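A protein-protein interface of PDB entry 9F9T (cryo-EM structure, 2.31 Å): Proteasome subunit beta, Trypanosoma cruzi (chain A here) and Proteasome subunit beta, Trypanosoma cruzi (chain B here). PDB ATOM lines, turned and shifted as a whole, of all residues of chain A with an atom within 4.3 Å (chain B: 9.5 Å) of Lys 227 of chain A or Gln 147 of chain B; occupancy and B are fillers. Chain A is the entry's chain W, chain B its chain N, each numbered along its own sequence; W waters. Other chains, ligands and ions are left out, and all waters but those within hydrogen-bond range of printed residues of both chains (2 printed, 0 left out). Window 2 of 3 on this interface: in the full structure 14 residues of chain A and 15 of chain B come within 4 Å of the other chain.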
ATOM      1  N   ALA A 199      22.385 -18.132  -4.828  1.00  0.00           N
ATOM      2  CA  ALA A 199      23.024 -17.030  -4.153  1.00  0.00           C
ATOM      3  C   ALA A 199      23.099 -15.815  -5.039  1.00  0.00           C
ATOM      4  O   ALA A 199      22.730 -14.734  -4.589  1.00  0.00           O
ATOM      5  CB  ALA A 199      24.389 -17.518  -3.792  1.00  0.00           C
ATOM      6  N   ALA A 200      23.612 -16.008  -6.262  1.00  0.00           N
ATOM      7  CA  ALA A 200      23.757 -14.925  -7.214  1.00  0.00           C
ATOM      8  C   ALA A 200      22.440 -14.209  -7.456  1.00  0.00           C
ATOM      9  O   ALA A 200      22.367 -13.013  -7.509  1.00  0.00           O
ATOM     10  CB  ALA A 200      24.202 -15.479  -8.505  1.00  0.00           C
ATOM     11  N   ALA A 203      21.249 -11.477  -5.185  1.00  0.00           N
ATOM     12  CA  ALA A 203      21.790 -10.148  -5.393  1.00  0.00           C
ATOM     13  C   ALA A 203      21.051  -9.462  -6.526  1.00  0.00           C
ATOM     14  O   ALA A 203      20.760  -8.292  -6.468  1.00  0.00           O
ATOM     15  CB  ALA A 203      23.255 -10.276  -5.689  1.00  0.00           C
ATOM     16  N   SER A 223      28.820  -8.111  -8.018  1.00  0.00           N
ATOM     17  CA  SER A 223      28.371  -8.412  -6.672  1.00  0.00           C
ATOM     18  C   SER A 223      27.646  -9.740  -6.688  1.00  0.00           C
ATOM     19  O   SER A 223      27.705 -10.463  -5.722  1.00  0.00           O
ATOM     20  CB  SER A 223      27.392  -7.336  -6.226  1.00  0.00           C
ATOM     21  OG  SER A 223      26.906  -7.672  -4.920  1.00  0.00           O
ATOM     22  N   ALA A 224      26.911 -10.017  -7.784  1.00  0.00           N
ATOM     23  CA  ALA A 224      26.202 -11.271  -7.884  1.00  0.00           C
ATOM     24  C   ALA A 224      27.167 -12.460  -7.979  1.00  0.00           C
ATOM     25  O   ALA A 224      26.954 -13.453  -7.313  1.00  0.00           O
ATOM     26  CB  ALA A 224      25.211 -11.242  -8.966  1.00  0.00           C
ATOM     27  N   ILE A 225      28.235 -12.356  -8.766  1.00  0.00           N
ATOM     28  CA  ILE A 225      29.266 -13.377  -8.827  1.00  0.00           C
ATOM     29  C   ILE A 225      29.925 -13.531  -7.460  1.00  0.00           C
ATOM     30  O   ILE A 225      30.159 -14.631  -7.071  1.00  0.00           O
ATOM     31  CB  ILE A 225      30.319 -13.047  -9.893  1.00  0.00           C
ATOM     32  CG1 ILE A 225      29.687 -12.879 -11.249  1.00  0.00           C
ATOM     33  CG2 ILE A 225      31.450 -14.107  -9.941  1.00  0.00           C
ATOM     34  CD1 ILE A 225      29.170 -14.206 -11.780  1.00  0.00           C
ATOM     35  N   ARG A 226      30.263 -12.458  -6.772  1.00  0.00           N
ATOM     36  CA  ARG A 226      30.920 -12.589  -5.467  1.00  0.00           C
ATOM     37  C   ARG A 226      30.047 -13.340  -4.454  1.00  0.00           C
ATOM     38  O   ARG A 226      30.549 -14.093  -3.635  1.00  0.00           O
ATOM     39  CB  ARG A 226      31.220 -11.260  -4.810  1.00  0.00           C
ATOM     40  CG  ARG A 226      32.400 -10.496  -5.407  1.00  0.00           C
ATOM     41  CD  ARG A 226      32.786  -9.273  -4.568  1.00  0.00           C
ATOM     42  NE  ARG A 226      31.771  -8.192  -4.616  1.00  0.00           N
ATOM     43  CZ  ARG A 226      31.702  -7.222  -5.544  1.00  0.00           C
ATOM     44  NH1 ARG A 226      30.688  -6.380  -5.574  1.00  0.00           N
ATOM     45  NH2 ARG A 226      32.626  -7.113  -6.475  1.00  0.00           N
ATOM     46  N   LYS A 227      28.728 -13.327  -4.635  1.00  0.00           N
ATOM     47  CA  LYS A 227      27.892 -14.120  -3.750  1.00  0.00           C
ATOM     48  C   LYS A 227      28.123 -15.597  -3.980  1.00  0.00           C
ATOM     49  O   LYS A 227      28.080 -16.402  -3.088  1.00  0.00           O
ATOM     50  CB  LYS A 227      26.404 -13.920  -4.038  1.00  0.00           C
ATOM     51  CG  LYS A 227      25.886 -12.512  -3.806  1.00  0.00           C
ATOM     52  CD  LYS A 227      25.693 -12.116  -2.394  1.00  0.00           C
ATOM     53  CE  LYS A 227      25.756 -10.613  -2.344  1.00  0.00           C
ATOM     54  NZ  LYS A 227      27.163 -10.250  -2.695  1.00  0.00           N
ATOM     55  N   GLY A 228      28.152 -15.984  -5.211  1.00  0.00           N
ATOM     56  CA  GLY A 228      28.594 -17.335  -5.503  1.00  0.00           C
ATOM     57  C   GLY A 228      29.959 -17.724  -4.921  1.00  0.00           C
ATOM     58  O   GLY A 228      30.065 -18.793  -4.366  1.00  0.00           O
ATOM     59  N   ILE A 229      30.993 -16.921  -5.223  1.00  0.00           N
ATOM     60  CA  ILE A 229      32.375 -17.155  -4.846  1.00  0.00           C
ATOM     61  C   ILE A 229      32.432 -17.456  -3.341  1.00  0.00           C
ATOM     62  O   ILE A 229      32.941 -18.503  -2.976  1.00  0.00           O
ATOM     63  CB  ILE A 229      33.245 -15.962  -5.307  1.00  0.00           C
ATOM     64  CG1 ILE A 229      33.392 -15.941  -6.837  1.00  0.00           C
ATOM     65  CG2 ILE A 229      34.592 -15.943  -4.622  1.00  0.00           C
ATOM     66  CD1 ILE A 229      34.176 -14.807  -7.428  1.00  0.00           C
ATOM     67  N   PHE A 230      31.787 -16.672  -2.498  1.00  0.00           N
ATOM     68  CA  PHE A 230      31.944 -16.815  -1.056  1.00  0.00           C
ATOM     69  C   PHE A 230      30.934 -17.747  -0.401  1.00  0.00           C
ATOM     70  O   PHE A 230      31.058 -17.986   0.768  1.00  0.00           O
ATOM     71  CB  PHE A 230      31.795 -15.472  -0.347  1.00  0.00           C
ATOM     72  CG  PHE A 230      32.951 -14.595  -0.720  1.00  0.00           C
ATOM     73  CD1 PHE A 230      34.257 -14.989  -0.410  1.00  0.00           C
ATOM     74  CD2 PHE A 230      32.767 -13.386  -1.347  1.00  0.00           C
ATOM     75  CE1 PHE A 230      35.339 -14.194  -0.760  1.00  0.00           C
ATOM     76  CE2 PHE A 230      33.852 -12.616  -1.746  1.00  0.00           C
ATOM     77  CZ  PHE A 230      35.128 -13.030  -1.467  1.00  0.00           C
ATOM     78  N   ASN A 231      29.966 -18.307  -1.106  1.00  0.00           N
ATOM     79  CA  ASN A 231      28.936 -19.030  -0.402  1.00  0.00           C
ATOM     80  C   ASN A 231      28.716 -20.412  -1.002  1.00  0.00           C
ATOM     81  O   ASN A 231      28.251 -21.298  -0.290  1.00  0.00           O
ATOM     82  CB  ASN A 231      27.630 -18.228  -0.351  1.00  0.00           C
ATOM     83  CG  ASN A 231      27.760 -16.890   0.359  1.00  0.00           C
ATOM     84  OD1 ASN A 231      27.703 -16.817   1.595  1.00  0.00           O
ATOM     85  ND2 ASN A 231      27.856 -15.818  -0.423  1.00  0.00           N
ATOM     86  N   VAL B  10      19.094 -12.793  12.222  1.00  0.00           N
ATOM     87  CA  VAL B  10      20.316 -11.998  12.165  1.00  0.00           C
ATOM     88  C   VAL B  10      20.519 -11.273  13.458  1.00  0.00           C
ATOM     89  O   VAL B  10      19.554 -10.823  14.010  1.00  0.00           O
ATOM     90  CB  VAL B  10      20.328 -11.020  10.974  1.00  0.00           C
ATOM     91  CG1 VAL B  10      19.333  -9.876  11.109  1.00  0.00           C
ATOM     92  CG2 VAL B  10      21.702 -10.491  10.673  1.00  0.00           C
ATOM     93  N   CYS B 131      24.455 -14.798  11.556  1.00  0.00           N
ATOM     94  CA  CYS B 131      23.304 -15.035  10.742  1.00  0.00           C
ATOM     95  C   CYS B 131      23.109 -16.511  10.482  1.00  0.00           C
ATOM     96  O   CYS B 131      24.053 -17.186  10.173  1.00  0.00           O
ATOM     97  CB  CYS B 131      23.447 -14.217   9.486  1.00  0.00           C
ATOM     98  SG  CYS B 131      24.691 -14.803   8.301  1.00  0.00           S
ATOM     99  N   ALA B 138      18.814 -20.749   3.659  1.00  0.00           N
ATOM    100  CA  ALA B 138      20.250 -20.949   3.671  1.00  0.00           C
ATOM    101  C   ALA B 138      20.909 -20.639   2.322  1.00  0.00           C
ATOM    102  O   ALA B 138      22.108 -20.334   2.310  1.00  0.00           O
ATOM    103  CB  ALA B 138      20.601 -22.309   4.085  1.00  0.00           C
ATOM    104  N   TYR B 139      20.163 -20.734   1.211  1.00  0.00           N
ATOM    105  CA  TYR B 139      20.762 -20.542  -0.094  1.00  0.00           C
ATOM    106  C   TYR B 139      20.509 -19.137  -0.555  1.00  0.00           C
ATOM    107  O   TYR B 139      21.374 -18.610  -1.241  1.00  0.00           O
ATOM    108  CB  TYR B 139      20.217 -21.590  -1.043  1.00  0.00           C
ATOM    109  CG  TYR B 139      20.543 -23.011  -0.611  1.00  0.00           C
ATOM    110  CD1 TYR B 139      21.850 -23.465  -0.653  1.00  0.00           C
ATOM    111  CD2 TYR B 139      19.568 -23.850  -0.060  1.00  0.00           C
ATOM    112  CE1 TYR B 139      22.177 -24.733  -0.193  1.00  0.00           C
ATOM    113  CE2 TYR B 139      19.877 -25.123   0.413  1.00  0.00           C
ATOM    114  CZ  TYR B 139      21.199 -25.569   0.342  1.00  0.00           C
ATOM    115  OH  TYR B 139      21.614 -26.829   0.736  1.00  0.00           O
ATOM    116  N   VAL B 140      19.387 -18.534  -0.160  1.00  0.00           N
ATOM    117  CA  VAL B 140      18.876 -17.291  -0.716  1.00  0.00           C
ATOM    118  C   VAL B 140      19.186 -16.108   0.217  1.00  0.00           C
ATOM    119  O   VAL B 140      19.586 -15.037  -0.222  1.00  0.00           O
ATOM    120  CB  VAL B 140      17.357 -17.391  -0.928  1.00  0.00           C
ATOM    121  CG1 VAL B 140      16.698 -16.036  -1.083  1.00  0.00           C
ATOM    122  CG2 VAL B 140      16.927 -18.233  -2.115  1.00  0.00           C
ATOM    123  N   ALA B 141      19.027 -16.298   1.517  1.00  0.00           N
ATOM    124  CA  ALA B 141      19.177 -15.228   2.477  1.00  0.00           C
ATOM    125  C   ALA B 141      20.594 -15.014   2.944  1.00  0.00           C
ATOM    126  O   ALA B 141      20.983 -13.884   3.131  1.00  0.00           O
ATOM    127  CB  ALA B 141      18.348 -15.549   3.686  1.00  0.00           C
ATOM    128  N   LEU B 142      21.255 -16.081   3.339  1.00  0.00           N
ATOM    129  CA  LEU B 142      22.570 -15.958   3.947  1.00  0.00           C
ATOM    130  C   LEU B 142      23.554 -15.156   3.112  1.00  0.00           C
ATOM    131  O   LEU B 142      24.311 -14.368   3.676  1.00  0.00           O
ATOM    132  CB  LEU B 142      23.177 -17.340   4.200  1.00  0.00           C
ATOM    133  CG  LEU B 142      22.579 -18.102   5.373  1.00  0.00           C
ATOM    134  CD1 LEU B 142      23.248 -19.450   5.517  1.00  0.00           C
ATOM    135  CD2 LEU B 142      22.664 -17.309   6.655  1.00  0.00           C
ATOM    136  N   PRO B 143      23.632 -15.315   1.782  1.00  0.00           N
ATOM    137  CA  PRO B 143      24.472 -14.420   0.984  1.00  0.00           C
ATOM    138  C   PRO B 143      24.206 -12.941   1.166  1.00  0.00           C
ATOM    139  O   PRO B 143      25.160 -12.190   1.266  1.00  0.00           O
ATOM    140  CB  PRO B 143      24.284 -14.866  -0.445  1.00  0.00           C
ATOM    141  CG  PRO B 143      23.943 -16.370  -0.287  1.00  0.00           C
ATOM    142  CD  PRO B 143      23.070 -16.401   0.971  1.00  0.00           C
ATOM    143  N   LEU B 144      22.963 -12.551   1.410  1.00  0.00           N
ATOM    144  CA  LEU B 144      22.685 -11.165   1.690  1.00  0.00           C
ATOM    145  C   LEU B 144      22.986 -10.717   3.105  1.00  0.00           C
ATOM    146  O   LEU B 144      23.308  -9.546   3.265  1.00  0.00           O
ATOM    147  CB  LEU B 144      21.210 -10.868   1.482  1.00  0.00           C
ATOM    148  CG  LEU B 144      20.664 -10.998   0.080  1.00  0.00           C
ATOM    149  CD1 LEU B 144      19.200 -10.573   0.068  1.00  0.00           C
ATOM    150  CD2 LEU B 144      21.462 -10.141  -0.905  1.00  0.00           C
ATOM    151  N   LEU B 145      22.641 -11.483   4.125  1.00  0.00           N
ATOM    152  CA  LEU B 145      22.899 -11.082   5.511  1.00  0.00           C
ATOM    153  C   LEU B 145      24.392 -11.054   5.691  1.00  0.00           C
ATOM    154  O   LEU B 145      24.899 -10.129   6.247  1.00  0.00           O
ATOM    155  CB  LEU B 145      22.308 -12.094   6.472  1.00  0.00           C
ATOM    156  CG  LEU B 145      20.847 -12.373   6.183  1.00  0.00           C
ATOM    157  CD1 LEU B 145      20.343 -13.584   6.984  1.00  0.00           C
ATOM    158  CD2 LEU B 145      20.027 -11.146   6.531  1.00  0.00           C
ATOM    159  N   ARG B 146      25.088 -12.039   5.092  1.00  0.00           N
ATOM    160  CA  ARG B 146      26.533 -12.082   5.251  1.00  0.00           C
ATOM    161  C   ARG B 146      27.170 -10.879   4.590  1.00  0.00           C
ATOM    162  O   ARG B 146      28.101 -10.342   5.138  1.00  0.00           O
ATOM    163  CB  ARG B 146      27.206 -13.357   4.728  1.00  0.00           C
ATOM    164  CG  ARG B 146      26.892 -14.555   5.599  1.00  0.00           C
ATOM    165  CD  ARG B 146      27.377 -15.821   4.897  1.00  0.00           C
ATOM    166  NE  ARG B 146      27.150 -16.967   5.735  1.00  0.00           N
ATOM    167  CZ  ARG B 146      27.153 -18.202   5.291  1.00  0.00           C
ATOM    168  NH1 ARG B 146      27.255 -18.444   3.981  1.00  0.00           N
ATOM    169  NH2 ARG B 146      26.943 -19.203   6.138  1.00  0.00           N
ATOM    170  N   GLN B 147      26.709 -10.465   3.435  1.00  0.00           N
ATOM    171  CA  GLN B 147      27.246  -9.259   2.822  1.00  0.00           C
ATOM    172  C   GLN B 147      27.001  -8.057   3.722  1.00  0.00           C
ATOM    173  O   GLN B 147      27.827  -7.179   3.797  1.00  0.00           O
ATOM    174  CB  GLN B 147      26.596  -9.017   1.446  1.00  0.00           C
ATOM    175  CG  GLN B 147      27.170  -7.856   0.642  1.00  0.00           C
ATOM    176  CD  GLN B 147      26.312  -7.523  -0.560  1.00  0.00           C
ATOM    177  OE1 GLN B 147      26.793  -7.473  -1.690  1.00  0.00           O
ATOM    178  NE2 GLN B 147      25.011  -7.337  -0.348  1.00  0.00           N
ATOM    179  N   ALA B 148      25.844  -8.018   4.368  1.00  0.00           N
ATOM    180  CA  ALA B 148      25.407  -6.865   5.139  1.00  0.00           C
ATOM    181  C   ALA B 148      26.278  -6.694   6.366  1.00  0.00           C
ATOM    182  O   ALA B 148      26.570  -5.569   6.727  1.00  0.00           O
ATOM    183  CB  ALA B 148      23.966  -7.029   5.596  1.00  0.00           C
ATOM    184  N   LEU B 149      26.647  -7.815   6.999  1.00  0.00           N
ATOM    185  CA  LEU B 149      27.416  -7.857   8.226  1.00  0.00           C
ATOM    186  C   LEU B 149      28.904  -7.616   8.007  1.00  0.00           C
ATOM    187  O   LEU B 149      29.628  -7.553   8.995  1.00  0.00           O
ATOM    188  CB  LEU B 149      27.275  -9.248   8.845  1.00  0.00           C
ATOM    189  CG  LEU B 149      25.957  -9.534   9.551  1.00  0.00           C
ATOM    190  CD1 LEU B 149      25.871 -10.984   9.924  1.00  0.00           C
ATOM    191  CD2 LEU B 149      25.840  -8.682  10.778  1.00  0.00           C
ATOM    192  N   GLU B 150      29.356  -7.626   6.753  1.00  0.00           N
ATOM    193  CA  GLU B 150      30.727  -7.286   6.394  1.00  0.00           C
ATOM    194  C   GLU B 150      31.075  -5.887   6.910  1.00  0.00           C
ATOM    195  O   GLU B 150      32.242  -5.639   7.196  1.00  0.00           O
ATOM    196  CB  GLU B 150      30.982  -7.291   4.867  1.00  0.00           C
ATOM    197  CG  GLU B 150      31.364  -8.640   4.241  1.00  0.00           C
ATOM    198  CD  GLU B 150      31.391  -8.687   2.702  1.00  0.00           C
ATOM    199  OE1 GLU B 150      30.894  -9.695   2.089  1.00  0.00           O
ATOM    200  OE2 GLU B 150      31.928  -7.728   2.092  1.00  0.00           O
ATOM    201  N   LYS B 151      30.113  -4.958   6.945  1.00  0.00           N
ATOM    202  CA  LYS B 151      30.396  -3.607   7.419  1.00  0.00           C
ATOM    203  C   LYS B 151      30.962  -3.673   8.835  1.00  0.00           C
ATOM    204  O   LYS B 151      30.566  -4.530   9.623  1.00  0.00           O
ATOM    205  CB  LYS B 151      29.181  -2.679   7.385  1.00  0.00           C
ATOM    206  CG  LYS B 151      28.278  -2.680   8.614  1.00  0.00           C
ATOM    207  CD  LYS B 151      27.307  -1.497   8.644  1.00  0.00           C
ATOM    208  CE  LYS B 151      27.994  -0.185   8.979  1.00  0.00           C
ATOM    209  NZ  LYS B 151      27.100   0.976   8.772  1.00  0.00           N
ATOM    210  N   PRO B 152      31.926  -2.794   9.195  1.00  0.00           N
ATOM    211  CA  PRO B 152      32.595  -2.896  10.494  1.00  0.00           C
ATOM    212  C   PRO B 152      31.792  -2.164  11.573  1.00  0.00           C
ATOM    213  O   PRO B 152      31.236  -1.086  11.330  1.00  0.00           O
ATOM    214  CB  PRO B 152      33.974  -2.294  10.177  1.00  0.00           C
ATOM    215  CG  PRO B 152      33.687  -1.231   9.111  1.00  0.00           C
ATOM    216  CD  PRO B 152      32.421  -1.658   8.392  1.00  0.00           C
ATOM    217  N   GLY B 154      29.079  -3.520  12.929  1.00  0.00           N
ATOM    218  CA  GLY B 154      27.819  -4.247  13.000  1.00  0.00           C
ATOM    219  C   GLY B 154      26.626  -3.434  12.506  1.00  0.00           C
ATOM    220  O   GLY B 154      26.775  -2.381  11.894  1.00  0.00           O
ATOM    221  N   LEU B 155      25.438  -3.958  12.770  1.00  0.00           N
ATOM    222  CA  LEU B 155      24.214  -3.449  12.186  1.00  0.00           C
ATOM    223  C   LEU B 155      23.383  -2.750  13.240  1.00  0.00           C
ATOM    224  O   LEU B 155      23.235  -3.303  14.322  1.00  0.00           O
ATOM    225  CB  LEU B 155      23.419  -4.651  11.667  1.00  0.00           C
ATOM    226  CG  LEU B 155      23.946  -5.403  10.461  1.00  0.00           C
ATOM    227  CD1 LEU B 155      23.015  -6.548  10.150  1.00  0.00           C
ATOM    228  CD2 LEU B 155      24.061  -4.519   9.228  1.00  0.00           C
ATOM    229  N   VAL B 163      17.465  -5.393   5.730  1.00  0.00           N
ATOM    230  CA  VAL B 163      18.090  -6.474   5.000  1.00  0.00           C
ATOM    231  C   VAL B 163      17.278  -7.750   5.215  1.00  0.00           C
ATOM    232  O   VAL B 163      17.210  -8.562   4.300  1.00  0.00           O
ATOM    233  CB  VAL B 163      19.584  -6.668   5.373  1.00  0.00           C
ATOM    234  CG1 VAL B 163      19.748  -7.019   6.863  1.00  0.00           C
ATOM    235  CG2 VAL B 163      20.275  -7.722   4.475  1.00  0.00           C
ATOM    236  N   ASP B 166      14.581  -7.500   2.444  1.00  0.00           N
ATOM    237  CA  ASP B 166      15.079  -7.834   1.122  1.00  0.00           C
ATOM    238  C   ASP B 166      15.186  -9.349   0.939  1.00  0.00           C
ATOM    239  O   ASP B 166      14.897  -9.864  -0.141  1.00  0.00           O
ATOM    240  CB  ASP B 166      16.422  -7.151   0.851  1.00  0.00           C
ATOM    241  CG  ASP B 166      16.344  -5.621   0.671  1.00  0.00           C
ATOM    242  OD1 ASP B 166      15.206  -5.034   0.764  1.00  0.00           O
ATOM    243  OD2 ASP B 166      17.421  -4.996   0.419  1.00  0.00           O
ATOM    244  N   CYS B 167      15.619 -10.061   2.001  1.00  0.00           N
ATOM    245  CA  CYS B 167      15.682 -11.520   1.940  1.00  0.00           C
ATOM    246  C   CYS B 167      14.263 -12.100   1.806  1.00  0.00           C
ATOM    247  O   CYS B 167      13.995 -12.971   0.981  1.00  0.00           O
ATOM    248  CB  CYS B 167      16.316 -12.105   3.199  1.00  0.00           C
ATOM    249  SG  CYS B 167      18.022 -11.600   3.559  1.00  0.00           S
HETATM  250  O   HOH W   1      26.866 -20.679   2.148  1.00  0.00           O
HETATM  251  O   HOH W   2      27.839 -13.172   1.025  1.00  0.00           O
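Water W2 bridges O of Pro 143 of chain B (2.9 Å) and ND2 of Asn 231 of chain A (3.0 Å). Water W1 bridges the backbone carbonyl oxygen of Asn 231 of chain A and the guanidinium group of Arg 146 of chain B.
Along chain B the printed residues that touch a printed residue of chain A span positions 139 to 147. Of the 12 printed residues of chain A, 4 touch a printed residue of chain B. Among the printed residues, no Asp or Glu carboxylate lies within 4 Å of a Lys or Arg side-chain nitrogen of the other chain.
Among the printed residues, merely in contact across the chains: Lys 227 of chain A with Pro 143 of chain B, Asn 231 of chain A with Pro 143 of chain B, Ala 199 of chain A with Tyr 139 of chain B and Ala 199 of chain A with Pro 143 of chain B.
The guanidinium group (NH1) of Arg 146 of chain B is in hydrogen-bond range of the side-chain amide oxygen (OD1) of Asn 231 of chain A (2.9 Å). The side-chain amide oxygen (OE1) of Gln 147 of chain B is in hydrogen-bond range of the side-chain hydroxyl (OG) of Ser 223 of chain A (3.2 Å). NZ of Lys 227 of chain A lies within hydrogen-bond range of OE1 of Gln 147 of chain B.
O of Ser 223 of chain A lies within hydrogen-bond range of NZ of Lys 227 of chain A, 3.1 Å away. O of Lys 227 of chain A sits at hydrogen-bond distance from ND2 of Asn 231 of chain A (2.7 Å).
Of the printed residues of chain B, Lys 227 of chain A touches Pro 143 (3.7 Å) and Gln 147 (3.0 Å). Of chain A, only Ser 223 and Lys 227 come within 4 Å of Gln 147 of chain B. No residue of chain B comes within 4 Å of Ala 200 of chain A. No residue of chain B comes within 4 Å of Ala 224 of chain A. No residue of chain B comes within 4 Å of Gly 228 of chain A. Of the printed residues of chain B, Ala 199 of chain A touches Tyr 139 and Pro 143. Of the printed residues of chain A, Tyr 139 of chain B touches Ala 199. Printed residues of chain B within 4 Å of Ser 223 of chain A: Gln 147. Of the printed residues of chain A, Pro 143 of chain B touches Ala 199, Lys 227 and Asn 231. Phe 230 of chain A touches none of the printed residues of chain B. The nearest residue of chain B that does not touch Lys 227 of chain A is Leu 144 of chain B (4.6 Å). The nearest printed residue of chain B that does not touch Asn 231 of chain A is Leu 142 of chain B (4.7 Å).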
